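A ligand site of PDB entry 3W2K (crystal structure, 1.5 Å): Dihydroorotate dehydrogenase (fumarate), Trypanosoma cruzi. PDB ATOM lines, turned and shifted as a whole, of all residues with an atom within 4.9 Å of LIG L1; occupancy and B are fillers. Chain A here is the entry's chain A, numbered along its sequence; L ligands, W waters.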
ATOM      1  N   ALA A  19      11.838   0.596  -8.526  1.00  0.00           N
ATOM      2  CA  ALA A  19      10.441   0.700  -8.150  1.00  0.00           C
ATOM      3  C   ALA A  19       9.621  -0.287  -8.919  1.00  0.00           C
ATOM      4  O   ALA A  19       9.872  -0.613 -10.069  1.00  0.00           O
ATOM      5  CB  ALA A  19      10.014   2.151  -8.482  1.00  0.00           C
ATOM      6  N   ALA A  20       8.617  -0.858  -8.277  1.00  0.00           N
ATOM      7  CA  ALA A  20       7.775  -1.807  -8.953  1.00  0.00           C
ATOM      8  C   ALA A  20       7.233  -1.189 -10.228  1.00  0.00           C
ATOM      9  O   ALA A  20       6.839  -0.045 -10.308  1.00  0.00           O
ATOM     10  CB  ALA A  20       6.625  -2.336  -8.054  1.00  0.00           C
ATOM     11  N   GLY A  21       7.195  -2.010 -11.240  1.00  0.00           N
ATOM     12  CA  GLY A  21       6.762  -1.597 -12.527  1.00  0.00           C
ATOM     13  C   GLY A  21       7.837  -1.254 -13.512  1.00  0.00           C
ATOM     14  O   GLY A  21       7.623  -1.293 -14.745  1.00  0.00           O
ATOM     15  N   VAL A  22       9.011  -0.908 -13.026  1.00  0.00           N
ATOM     16  CA  VAL A  22      10.139  -0.521 -13.870  1.00  0.00           C
ATOM     17  C   VAL A  22      11.210  -1.620 -13.896  1.00  0.00           C
ATOM     18  O   VAL A  22      11.664  -2.030 -12.907  1.00  0.00           O
ATOM     19  CB  VAL A  22      10.725   0.838 -13.423  1.00  0.00           C
ATOM     20  CG1 VAL A  22      11.902   1.188 -14.312  1.00  0.00           C
ATOM     21  CG2 VAL A  22       9.657   1.886 -13.488  1.00  0.00           C
ATOM     22  N   LYS A  44       7.331  -6.830 -11.039  1.00  0.00           N
ATOM     23  CA  LYS A  44       6.120  -6.112 -11.486  1.00  0.00           C
ATOM     24  C   LYS A  44       4.886  -6.549 -10.710  1.00  0.00           C
ATOM     25  O   LYS A  44       4.650  -7.759 -10.624  1.00  0.00           O
ATOM     26  CB  LYS A  44       5.949  -6.431 -12.979  1.00  0.00           C
ATOM     27  CG  LYS A  44       4.697  -5.887 -13.571  1.00  0.00           C
ATOM     28  CD  LYS A  44       4.503  -4.359 -13.639  1.00  0.00           C
ATOM     29  CE  LYS A  44       3.058  -3.858 -13.817  1.00  0.00           C
ATOM     30  NZ  LYS A  44       2.800  -2.270 -13.954  1.00  0.00           N
ATOM     31  N   SER A  45       4.103  -5.578 -10.253  1.00  0.00           N
ATOM     32  CA  SER A  45       2.836  -5.892  -9.558  1.00  0.00           C
ATOM     33  C   SER A  45       2.052  -6.801 -10.464  1.00  0.00           C
ATOM     34  O   SER A  45       1.870  -6.539 -11.651  1.00  0.00           O
ATOM     35  CB  SER A  45       1.986  -4.679  -9.284  1.00  0.00           C
ATOM     36  OG  SER A  45       2.709  -3.892  -8.293  1.00  0.00           O
ATOM     37  N   TYR A  59       3.010   5.249 -21.553  1.00  0.00           N
ATOM     38  CA  TYR A  59       4.066   5.874 -20.747  1.00  0.00           C
ATOM     39  C   TYR A  59       4.790   6.913 -21.556  1.00  0.00           C
ATOM     40  O   TYR A  59       5.102   6.656 -22.659  1.00  0.00           O
ATOM     41  CB  TYR A  59       5.125   4.844 -20.309  1.00  0.00           C
ATOM     42  CG  TYR A  59       6.404   5.417 -19.656  1.00  0.00           C
ATOM     43  CD1 TYR A  59       6.463   5.659 -18.302  1.00  0.00           C
ATOM     44  CD2 TYR A  59       7.526   5.702 -20.390  1.00  0.00           C
ATOM     45  CE1 TYR A  59       7.570   6.150 -17.687  1.00  0.00           C
ATOM     46  CE2 TYR A  59       8.611   6.251 -19.795  1.00  0.00           C
ATOM     47  CZ  TYR A  59       8.669   6.433 -18.441  1.00  0.00           C
ATOM     48  OH  TYR A  59       9.826   6.916 -17.871  1.00  0.00           O
ATOM     49  N   SER A  66       7.639  11.713 -15.509  1.00  0.00           N
ATOM     50  CA  SER A  66       6.962  10.797 -16.362  1.00  0.00           C
ATOM     51  C   SER A  66       5.463  10.811 -15.991  1.00  0.00           C
ATOM     52  O   SER A  66       5.021  11.189 -14.904  1.00  0.00           O
ATOM     53  CB  SER A  66       7.501   9.369 -16.242  1.00  0.00           C
ATOM     54  OG  SER A  66       7.186   8.854 -14.945  1.00  0.00           O
ATOM     55  N   ASN A  68       2.135   7.868 -16.629  1.00  0.00           N
ATOM     56  CA  ASN A  68       1.843   6.512 -17.115  1.00  0.00           C
ATOM     57  C   ASN A  68       0.380   6.152 -16.764  1.00  0.00           C
ATOM     58  O   ASN A  68      -0.138   6.487 -15.689  1.00  0.00           O
ATOM     59  CB  ASN A  68       2.763   5.430 -16.613  1.00  0.00           C
ATOM     60  CG  ASN A  68       2.387   4.907 -15.280  1.00  0.00           C
ATOM     61  OD1 ASN A  68       1.544   3.954 -15.163  1.00  0.00           O
ATOM     62  ND2 ASN A  68       3.010   5.422 -14.222  1.00  0.00           N
ATOM     63  N   MET A  70      -0.385   2.553 -17.421  1.00  0.00           N
ATOM     64  CA  MET A  70      -0.040   1.255 -17.990  1.00  0.00           C
ATOM     65  C   MET A  70      -1.174   0.237 -18.038  1.00  0.00           C
ATOM     66  O   MET A  70      -1.267  -0.510 -18.970  1.00  0.00           O
ATOM     67  CB  MET A  70       1.124   0.630 -17.288  1.00  0.00           C
ATOM     68  CG  MET A  70       2.347   1.462 -17.127  1.00  0.00           C
ATOM     69  SD  MET A  70       3.110   1.911 -18.724  1.00  0.00           S
ATOM     70  CE  MET A  70       3.805   0.330 -19.258  1.00  0.00           C
ATOM     71  N   LEU A  72      -1.581  -2.140 -15.648  1.00  0.00           N
ATOM     72  CA  LEU A  72      -1.051  -3.316 -15.042  1.00  0.00           C
ATOM     73  C   LEU A  72      -0.746  -4.451 -15.989  1.00  0.00           C
ATOM     74  O   LEU A  72      -1.111  -5.551 -15.756  1.00  0.00           O
ATOM     75  CB  LEU A  72      -2.006  -3.749 -13.930  1.00  0.00           C
ATOM     76  CG  LEU A  72      -1.587  -4.630 -12.771  1.00  0.00           C
ATOM     77  CD1 LEU A  72      -0.395  -3.972 -12.108  1.00  0.00           C
ATOM     78  CD2 LEU A  72      -2.771  -4.569 -11.807  1.00  0.00           C
ATOM     79  N   SER A  98       5.837  -8.032  -5.851  1.00  0.00           N
ATOM     80  CA  SER A  98       4.714  -7.154  -5.663  1.00  0.00           C
ATOM     81  C   SER A  98       3.430  -7.766  -6.223  1.00  0.00           C
ATOM     82  O   SER A  98       3.452  -8.333  -7.319  1.00  0.00           O
ATOM     83  CB  SER A  98       4.972  -5.815  -6.359  1.00  0.00           C
ATOM     84  OG  SER A  98       3.795  -4.984  -6.253  1.00  0.00           O
ATOM     85  N   GLU A 126       5.492  -7.314  -1.266  1.00  0.00           N
ATOM     86  CA  GLU A 126       5.046  -5.886  -1.309  1.00  0.00           C
ATOM     87  C   GLU A 126       3.639  -5.921  -1.882  1.00  0.00           C
ATOM     88  O   GLU A 126       3.378  -6.168  -3.062  1.00  0.00           O
ATOM     89  CB  GLU A 126       5.958  -4.939  -2.129  1.00  0.00           C
ATOM     90  CG  GLU A 126       5.574  -3.431  -2.053  1.00  0.00           C
ATOM     91  CD  GLU A 126       6.624  -2.481  -2.781  1.00  0.00           C
ATOM     92  OE1 GLU A 126       6.455  -2.314  -4.008  1.00  0.00           O
ATOM     93  OE2 GLU A 126       7.581  -1.891  -2.170  1.00  0.00           O
ATOM     94  N   ASN A 128       0.565  -3.898  -3.192  1.00  0.00           N
ATOM     95  CA  ASN A 128       0.255  -2.601  -3.739  1.00  0.00           C
ATOM     96  C   ASN A 128      -1.188  -2.201  -3.476  1.00  0.00           C
ATOM     97  O   ASN A 128      -2.086  -2.761  -4.031  1.00  0.00           O
ATOM     98  CB  ASN A 128       0.479  -2.714  -5.233  1.00  0.00           C
ATOM     99  CG  ASN A 128       0.231  -1.420  -5.970  1.00  0.00           C
ATOM    100  OD1 ASN A 128      -0.022  -0.480  -5.420  1.00  0.00           O
ATOM    101  ND2 ASN A 128       0.373  -1.470  -7.270  1.00  0.00           N
ATOM    102  N   LYS A 165       2.752  -0.930  -0.471  1.00  0.00           N
ATOM    103  CA  LYS A 165       3.086   0.237  -1.300  1.00  0.00           C
ATOM    104  C   LYS A 165       1.879   1.178  -1.234  1.00  0.00           C
ATOM    105  O   LYS A 165       0.727   0.817  -1.546  1.00  0.00           O
ATOM    106  CB  LYS A 165       3.326  -0.236  -2.712  1.00  0.00           C
ATOM    107  CG  LYS A 165       3.611   0.839  -3.749  1.00  0.00           C
ATOM    108  CD  LYS A 165       4.977   1.420  -3.719  1.00  0.00           C
ATOM    109  CE  LYS A 165       5.356   2.282  -4.883  1.00  0.00           C
ATOM    110  NZ  LYS A 165       5.585   1.462  -6.065  1.00  0.00           N
ATOM    111  N   VAL A 194       6.457   6.580  -2.111  1.00  0.00           N
ATOM    112  CA  VAL A 194       5.100   6.546  -2.599  1.00  0.00           C
ATOM    113  C   VAL A 194       4.971   5.994  -4.009  1.00  0.00           C
ATOM    114  O   VAL A 194       5.877   5.922  -4.722  1.00  0.00           O
ATOM    115  CB  VAL A 194       4.491   7.993  -2.638  1.00  0.00           C
ATOM    116  CG1 VAL A 194       4.396   8.550  -1.253  1.00  0.00           C
ATOM    117  CG2 VAL A 194       5.293   8.933  -3.525  1.00  0.00           C
ATOM    118  N   ASN A 195       3.771   5.587  -4.308  1.00  0.00           N
ATOM    119  CA  ASN A 195       3.386   5.299  -5.686  1.00  0.00           C
ATOM    120  C   ASN A 195       3.235   6.659  -6.422  1.00  0.00           C
ATOM    121  O   ASN A 195       3.421   7.660  -5.874  1.00  0.00           O
ATOM    122  CB  ASN A 195       2.067   4.527  -5.701  1.00  0.00           C
ATOM    123  CG  ASN A 195       1.966   3.561  -6.855  1.00  0.00           C
ATOM    124  OD1 ASN A 195       2.166   3.926  -7.946  1.00  0.00           O
ATOM    125  ND2 ASN A 195       1.634   2.334  -6.567  1.00  0.00           N
ATOM    126  N   SER A 196       2.889   6.588  -7.693  1.00  0.00           N
ATOM    127  CA  SER A 196       2.773   7.796  -8.490  1.00  0.00           C
ATOM    128  C   SER A 196       1.700   8.778  -7.979  1.00  0.00           C
ATOM    129  O   SER A 196       0.791   8.402  -7.360  1.00  0.00           O
ATOM    130  CB  SER A 196       2.550   7.445  -9.969  1.00  0.00           C
ATOM    131  OG  SER A 196       1.557   6.540 -10.140  1.00  0.00           O
ATOM    132  N   GLY A 222       5.442  10.525 -12.022  1.00  0.00           N
ATOM    133  CA  GLY A 222       6.669  10.259 -11.351  1.00  0.00           C
ATOM    134  C   GLY A 222       7.759  11.223 -11.685  1.00  0.00           C
ATOM    135  O   GLY A 222       7.613  12.074 -12.586  1.00  0.00           O
ATOM    136  N   GLY A 223       8.903  11.092 -10.983  1.00  0.00           N
ATOM    137  CA  GLY A 223      10.084  11.816 -11.238  1.00  0.00           C
ATOM    138  C   GLY A 223      10.235  13.153 -10.483  1.00  0.00           C
ATOM    139  O   GLY A 223       9.799  13.241  -9.348  1.00  0.00           O
ATOM    140  N   ILE A 226       7.621  14.969  -8.224  1.00  0.00           N
ATOM    141  CA  ILE A 226       7.046  14.347  -7.005  1.00  0.00           C
ATOM    142  C   ILE A 226       8.007  14.247  -5.821  1.00  0.00           C
ATOM    143  O   ILE A 226       7.554  13.744  -4.795  1.00  0.00           O
ATOM    144  CB  ILE A 226       6.369  13.037  -7.325  1.00  0.00           C
ATOM    145  CG1 ILE A 226       7.296  11.851  -7.489  1.00  0.00           C
ATOM    146  CG2 ILE A 226       5.442  13.180  -8.529  1.00  0.00           C
ATOM    147  CD1 ILE A 226       6.574  10.514  -7.316  1.00  0.00           C
ATOM    148  N   CYS A 249      10.273   6.056  -2.154  1.00  0.00           N
ATOM    149  CA  CYS A 249      10.145   5.997  -3.609  1.00  0.00           C
ATOM    150  C   CYS A 249       9.585   7.345  -4.092  1.00  0.00           C
ATOM    151  O   CYS A 249       8.671   7.804  -3.614  1.00  0.00           O
ATOM    152  CB  CYS A 249       9.261   4.816  -3.989  1.00  0.00           C
ATOM    153  SG  CYS A 249       9.229   4.535  -5.825  1.00  0.00           S
ATOM    154  N   GLY A 250      10.241   7.906  -5.064  1.00  0.00           N
ATOM    155  CA  GLY A 250       9.764   9.110  -5.750  1.00  0.00           C
ATOM    156  C   GLY A 250      10.801  10.129  -5.972  1.00  0.00           C
ATOM    157  O   GLY A 250      11.342  10.688  -5.047  1.00  0.00           O
ATOM    158  N   GLY A 251      10.973  10.486  -7.243  1.00  0.00           N
ATOM    159  CA  GLY A 251      11.870  11.609  -7.573  1.00  0.00           C
ATOM    160  C   GLY A 251      13.336  11.361  -7.358  1.00  0.00           C
ATOM    161  O   GLY A 251      14.115  12.337  -7.317  1.00  0.00           O
ATOM    162  N   VAL A 252      13.811  10.114  -7.227  1.00  0.00           N
ATOM    163  CA  VAL A 252      15.269   9.860  -7.074  1.00  0.00           C
ATOM    164  C   VAL A 252      15.975   9.816  -8.407  1.00  0.00           C
ATOM    165  O   VAL A 252      15.723   8.939  -9.196  1.00  0.00           O
ATOM    166  CB  VAL A 252      15.533   8.573  -6.264  1.00  0.00           C
ATOM    167  CG1 VAL A 252      17.055   8.223  -6.147  1.00  0.00           C
ATOM    168  CG2 VAL A 252      14.891   8.646  -4.862  1.00  0.00           C
ATOM    169  N   GLN A 270      13.886   3.318  -3.606  1.00  0.00           N
ATOM    170  CA  GLN A 270      13.448   2.738  -4.893  1.00  0.00           C
ATOM    171  C   GLN A 270      13.593   3.837  -5.964  1.00  0.00           C
ATOM    172  O   GLN A 270      13.347   5.067  -5.714  1.00  0.00           O
ATOM    173  CB  GLN A 270      11.995   2.222  -4.841  1.00  0.00           C
ATOM    174  CG  GLN A 270      11.785   1.308  -3.652  1.00  0.00           C
ATOM    175  CD  GLN A 270      10.431   0.633  -3.681  1.00  0.00           C
ATOM    176  OE1 GLN A 270       9.521   1.195  -4.325  1.00  0.00           O
ATOM    177  NE2 GLN A 270      10.291  -0.478  -3.029  1.00  0.00           N
ATOM    178  N   VAL A 271      13.830   3.417  -7.203  1.00  0.00           N
ATOM    179  CA  VAL A 271      14.086   4.257  -8.361  1.00  0.00           C
ATOM    180  C   VAL A 271      13.223   3.766  -9.501  1.00  0.00           C
ATOM    181  O   VAL A 271      13.353   2.636  -9.971  1.00  0.00           O
ATOM    182  CB  VAL A 271      15.562   4.179  -8.751  1.00  0.00           C
ATOM    183  CG1 VAL A 271      15.814   5.241  -9.769  1.00  0.00           C
ATOM    184  CG2 VAL A 271      16.475   4.383  -7.507  1.00  0.00           C
ATOM    185  N   GLY A 272      12.336   4.638  -9.898  1.00  0.00           N
ATOM    186  CA  GLY A 272      11.361   4.373 -10.975  1.00  0.00           C
ATOM    187  C   GLY A 272      11.736   5.097 -12.259  1.00  0.00           C
ATOM    188  O   GLY A 272      12.528   4.626 -13.059  1.00  0.00           O
ATOM    189  N   THR A 273      11.145   6.262 -12.454  1.00  0.00           N
ATOM    190  CA  THR A 273      11.349   7.036 -13.663  1.00  0.00           C
ATOM    191  C   THR A 273      12.787   7.208 -14.056  1.00  0.00           C
ATOM    192  O   THR A 273      13.178   7.004 -15.197  1.00  0.00           O
ATOM    193  CB  THR A 273      10.756   8.444 -13.490  1.00  0.00           C
ATOM    194  OG1 THR A 273       9.331   8.340 -13.260  1.00  0.00           O
ATOM    195  CG2 THR A 273      10.933   9.345 -14.701  1.00  0.00           C
ATOM    196  N   ALA A 274      13.661   7.526 -13.118  1.00  0.00           N
ATOM    197  CA  ALA A 274      15.070   7.736 -13.470  1.00  0.00           C
ATOM    198  C   ALA A 274      15.726   6.489 -14.015  1.00  0.00           C
ATOM    199  O   ALA A 274      16.600   6.565 -14.874  1.00  0.00           O
ATOM    200  CB  ALA A 274      15.901   8.301 -12.295  1.00  0.00           C
HETATM  201  N1  LIG L   1       3.996   0.939  -8.746  1.00  0.00           N
HETATM  202  C1  LIG L   1       3.568  -0.258  -8.312  1.00  0.00           C
HETATM  203  O1  LIG L   1       3.593  -0.414  -7.050  1.00  0.00           O
HETATM  204  N2  LIG L   1       3.336  -1.312  -9.120  1.00  0.00           N
HETATM  205  C2  LIG L   1       3.423  -1.236 -10.471  1.00  0.00           C
HETATM  206  O2  LIG L   1       3.178  -2.225 -11.198  1.00  0.00           O
HETATM  207  C3  LIG L   1       3.848  -0.007 -11.018  1.00  0.00           C
HETATM  208  N3  LIG L   1       3.961   0.170 -12.343  1.00  0.00           N
HETATM  209  C4  LIG L   1       4.588   1.284 -12.827  1.00  0.00           C
HETATM  210  C5  LIG L   1       4.928   1.404 -14.177  1.00  0.00           C
HETATM  211  C6  LIG L   1       5.554   2.511 -14.709  1.00  0.00           C
HETATM  212  C7  LIG L   1       5.932   2.543 -16.179  1.00  0.00           C
HETATM  213  C8  LIG L   1       5.958   3.587 -13.821  1.00  0.00           C
HETATM  214  C9  LIG L   1       6.638   4.847 -14.328  1.00  0.00           C
HETATM  215  C10 LIG L   1       5.635   3.443 -12.480  1.00  0.00           C
HETATM  216  C11 LIG L   1       5.000   2.307 -11.918  1.00  0.00           C
HETATM  217  N4  LIG L   1       4.639   2.220 -10.540  1.00  0.00           N
HETATM  218  C12 LIG L   1       4.136   1.052 -10.046  1.00  0.00           C
HETATM  219  C13 LIG L   1       5.009   3.311  -9.616  1.00  0.00           C
HETATM  220  C14 LIG L   1       6.487   3.318  -9.296  1.00  0.00           C
HETATM  221  O3  LIG L   1       6.752   2.116  -8.593  1.00  0.00           O
HETATM  222  C15 LIG L   1       6.834   4.488  -8.400  1.00  0.00           C
HETATM  223  O4  LIG L   1       6.059   4.424  -7.214  1.00  0.00           O
HETATM  224  C16 LIG L   1       6.528   5.850  -9.063  1.00  0.00           C
HETATM  225  O5  LIG L   1       6.957   5.803 -10.456  1.00  0.00           O
HETATM  226  C17 LIG L   1       7.322   7.010  -8.393  1.00  0.00           C
HETATM  227  O6  LIG L   1       8.703   6.817  -8.392  1.00  0.00           O
HETATM  228  P1  LIG L   1       9.632   7.672  -9.393  1.00  0.00           P
HETATM  229  O7  LIG L   1      11.027   7.149  -9.169  1.00  0.00           O
HETATM  230  O8  LIG L   1       9.437   9.134  -9.108  1.00  0.00           O
HETATM  231  O9  LIG L   1       9.113   7.338 -10.823  1.00  0.00           O
HETATM  232  O1  LG2 L   2       0.116  -0.442 -14.156  1.00  0.00           O
HETATM  233  C1  LG2 L   2      -0.152   0.739 -13.828  1.00  0.00           C
HETATM  234  O2  LG2 L   2      -0.766   1.544 -14.513  1.00  0.00           O
HETATM  235  C2  LG2 L   2       0.426   1.295 -12.506  1.00  0.00           C
HETATM  236  N1  LG2 L   2       1.080   2.565 -12.671  1.00  0.00           N
HETATM  237  C3  LG2 L   2       1.552   3.267 -11.559  1.00  0.00           C
HETATM  238  O3  LG2 L   2       2.142   4.342 -11.694  1.00  0.00           O
HETATM  239  N2  LG2 L   2       1.386   2.617 -10.307  1.00  0.00           N
HETATM  240  C4  LG2 L   2       0.706   1.389 -10.135  1.00  0.00           C
HETATM  241  O4  LG2 L   2       0.565   0.945  -8.956  1.00  0.00           O
HETATM  242  C5  LG2 L   2       0.178   0.809 -11.264  1.00  0.00           C
HETATM  243  C6  LG2 L   2      -0.536  -0.412 -11.146  1.00  0.00           C
HETATM  244  C7  LG2 L   2      -1.896  -0.164 -10.359  1.00  0.00           C
HETATM  245  C8  LG2 L   2      -2.821  -0.017 -11.222  1.00  0.00           C
HETATM  246  C9  LG2 L   2      -3.464  -1.217 -11.513  1.00  0.00           C
HETATM  247  C10 LG2 L   2      -4.397  -1.281 -12.467  1.00  0.00           C
HETATM  248  C11 LG2 L   2      -5.069  -2.536 -12.700  1.00  0.00           C
HETATM  249  C12 LG2 L   2      -4.751  -0.082 -13.134  1.00  0.00           C
HETATM  250  F1  LG2 L   2      -5.721  -0.145 -14.068  1.00  0.00           F
HETATM  251  C13 LG2 L   2      -4.133   1.161 -12.878  1.00  0.00           C
HETATM  252  C14 LG2 L   2      -3.136   1.192 -11.879  1.00  0.00           C
HETATM  253  O   HOH W   1       4.145  -2.592  -5.250  1.00  0.00           O
HETATM  254  O   HOH W   2      13.090   8.367 -10.453  1.00  0.00           O
HETATM  255  O   HOH W   3       4.993   6.977 -11.661  1.00  0.00           O
HETATM  256  O   HOH W   4       4.982  -1.581 -15.974  1.00  0.00           O
HETATM  257  O   HOH W   5      12.420   7.424  -6.864  1.00  0.00           O
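The backbone NH of Thr 273 is in hydrogen-bond range of an oxygen (O9) of LIG L1 (2.8 Å). O9 of LIG L1 lies within hydrogen-bond range of OG1 of Thr 273 (2.6 Å). An oxygen (O3) of LIG L1 lies within hydrogen-bond range of the backbone carbonyl oxygen of Ala 20 (2.8 Å). The backbone NH (N) of Gly 223 lies within hydrogen-bond range of an oxygen (O8) of LIG L1 (2.8 Å). An oxygen (O8) of LIG L1 sits at hydrogen-bond distance from the backbone NH of Gly 251 (2.8 Å). The side-chain hydroxyl (OG) of Ser 45 lies within hydrogen-bond range of a nitrogen (N2) of LIG L1, 2.8 Å away. An oxygen (O2) of LIG L1 lies within hydrogen-bond range of the side-chain amino group of Lys 44 (2.8 Å). The side-chain amino group of Lys 165 lies within hydrogen-bond range of an oxygen (O3) of LIG L1, 2.9 Å away. O of Val 194 sits at hydrogen-bond distance from O4 of LIG L1. The backbone NH of Gly 272 sits at hydrogen-bond distance from an oxygen (O7) of LIG L1 (2.9 Å). ND2 of Asn 195 is in hydrogen-bond range of O1 of LIG L1 (3.4 Å). The side-chain amide nitrogen (ND2) of Asn 128 is in hydrogen-bond range of an oxygen (O1) of LIG L1, 3.4 Å away. SG of Cys 249 sits at hydrogen-bond distance from O4 of LIG L1 (3.5 Å). O1 of LG2 L2 lies within salt-bridge range of NZ of Lys 44 (3.3 Å). The side-chain amide oxygen of Asn 195 sits at hydrogen-bond distance from a nitrogen (N2) of LG2 L2 (2.8 Å). An oxygen (O4) of LG2 L2 lies within hydrogen-bond range of the side-chain amide nitrogen (ND2) of Asn 128 (3.0 Å). The side-chain amide nitrogen (ND2) of Asn 68 is in hydrogen-bond range of an oxygen (O3) of LG2 L2 (2.9 Å). N of Met 70 is in hydrogen-bond range of O2 of LG2 L2. OG of Ser 196 sits at hydrogen-bond distance from O3 of LG2 L2, 2.8 Å away. N of Leu 72 sits at hydrogen-bond distance from O1 of LG2 L2, 2.8 Å away.
A nitrogen (N1) of LIG L1 lies close to a nitrogen (N2) of LG2 L2 (3.5 Å).
The side-chain hydroxyl (OG1) of Thr 273 sits at hydrogen-bond distance from the side-chain hydroxyl (OG) of Ser 66, at 2.8 Å. N of Val 194 sits at hydrogen-bond distance from O of Cys 249 (2.9 Å). The side-chain amide nitrogen (ND2) of Asn 195 sits at hydrogen-bond distance from the side-chain amide oxygen (OD1) of Asn 128 (3.5 Å). OD1 of Asn 195 sits at hydrogen-bond distance from OG of Ser 196, at 3.5 Å. The backbone NH (N) of Ala 19 lies within hydrogen-bond range of the backbone carbonyl oxygen (O) of Val 271 (2.9 Å). The side-chain amide oxygen (OE1) of Gln 270 lies close to the side-chain sulfur (SG) of Cys 249, at 3.7 Å. The backbone NH (N) of Met 70 sits close to the side-chain amide oxygen (OD1) of Asn 68 (3.3 Å). O of Gly 222 sits at hydrogen-bond distance from N of Ser 66 (2.9 Å).
Merely in contact with LIG L1: Ala 19 (3.3 Å), Gly 21 (3.3 Å), Tyr 59 (3.7 Å), Asn 68 (3.5 Å), Met 70 (3.9 Å), Ser 196 (3.9 Å), Gly 222 (3.7 Å), Ile 226 (3.6 Å) and Gly 250 (3.4 Å). Hydrophobic or aromatic side chains within 4 Å of LIG L1: Ala 19, Ala 20, Tyr 59, Met 70 and Ile 226.
Water W2 lies within hydrogen-bond range of O7 of LIG L1, N of Ala 274, O of Val 252 and N of Thr 273. Water W1 lies within hydrogen-bond range of the side-chain hydroxyl of Ser 98, the side-chain carboxylate of Glu 126 and an oxygen (O1) of LIG L1. Water W4 lies within hydrogen-bond range of the backbone carbonyl oxygen of Gly 21 (2.9 Å) and the side-chain amino group of Lys 44 (3.1 Å).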
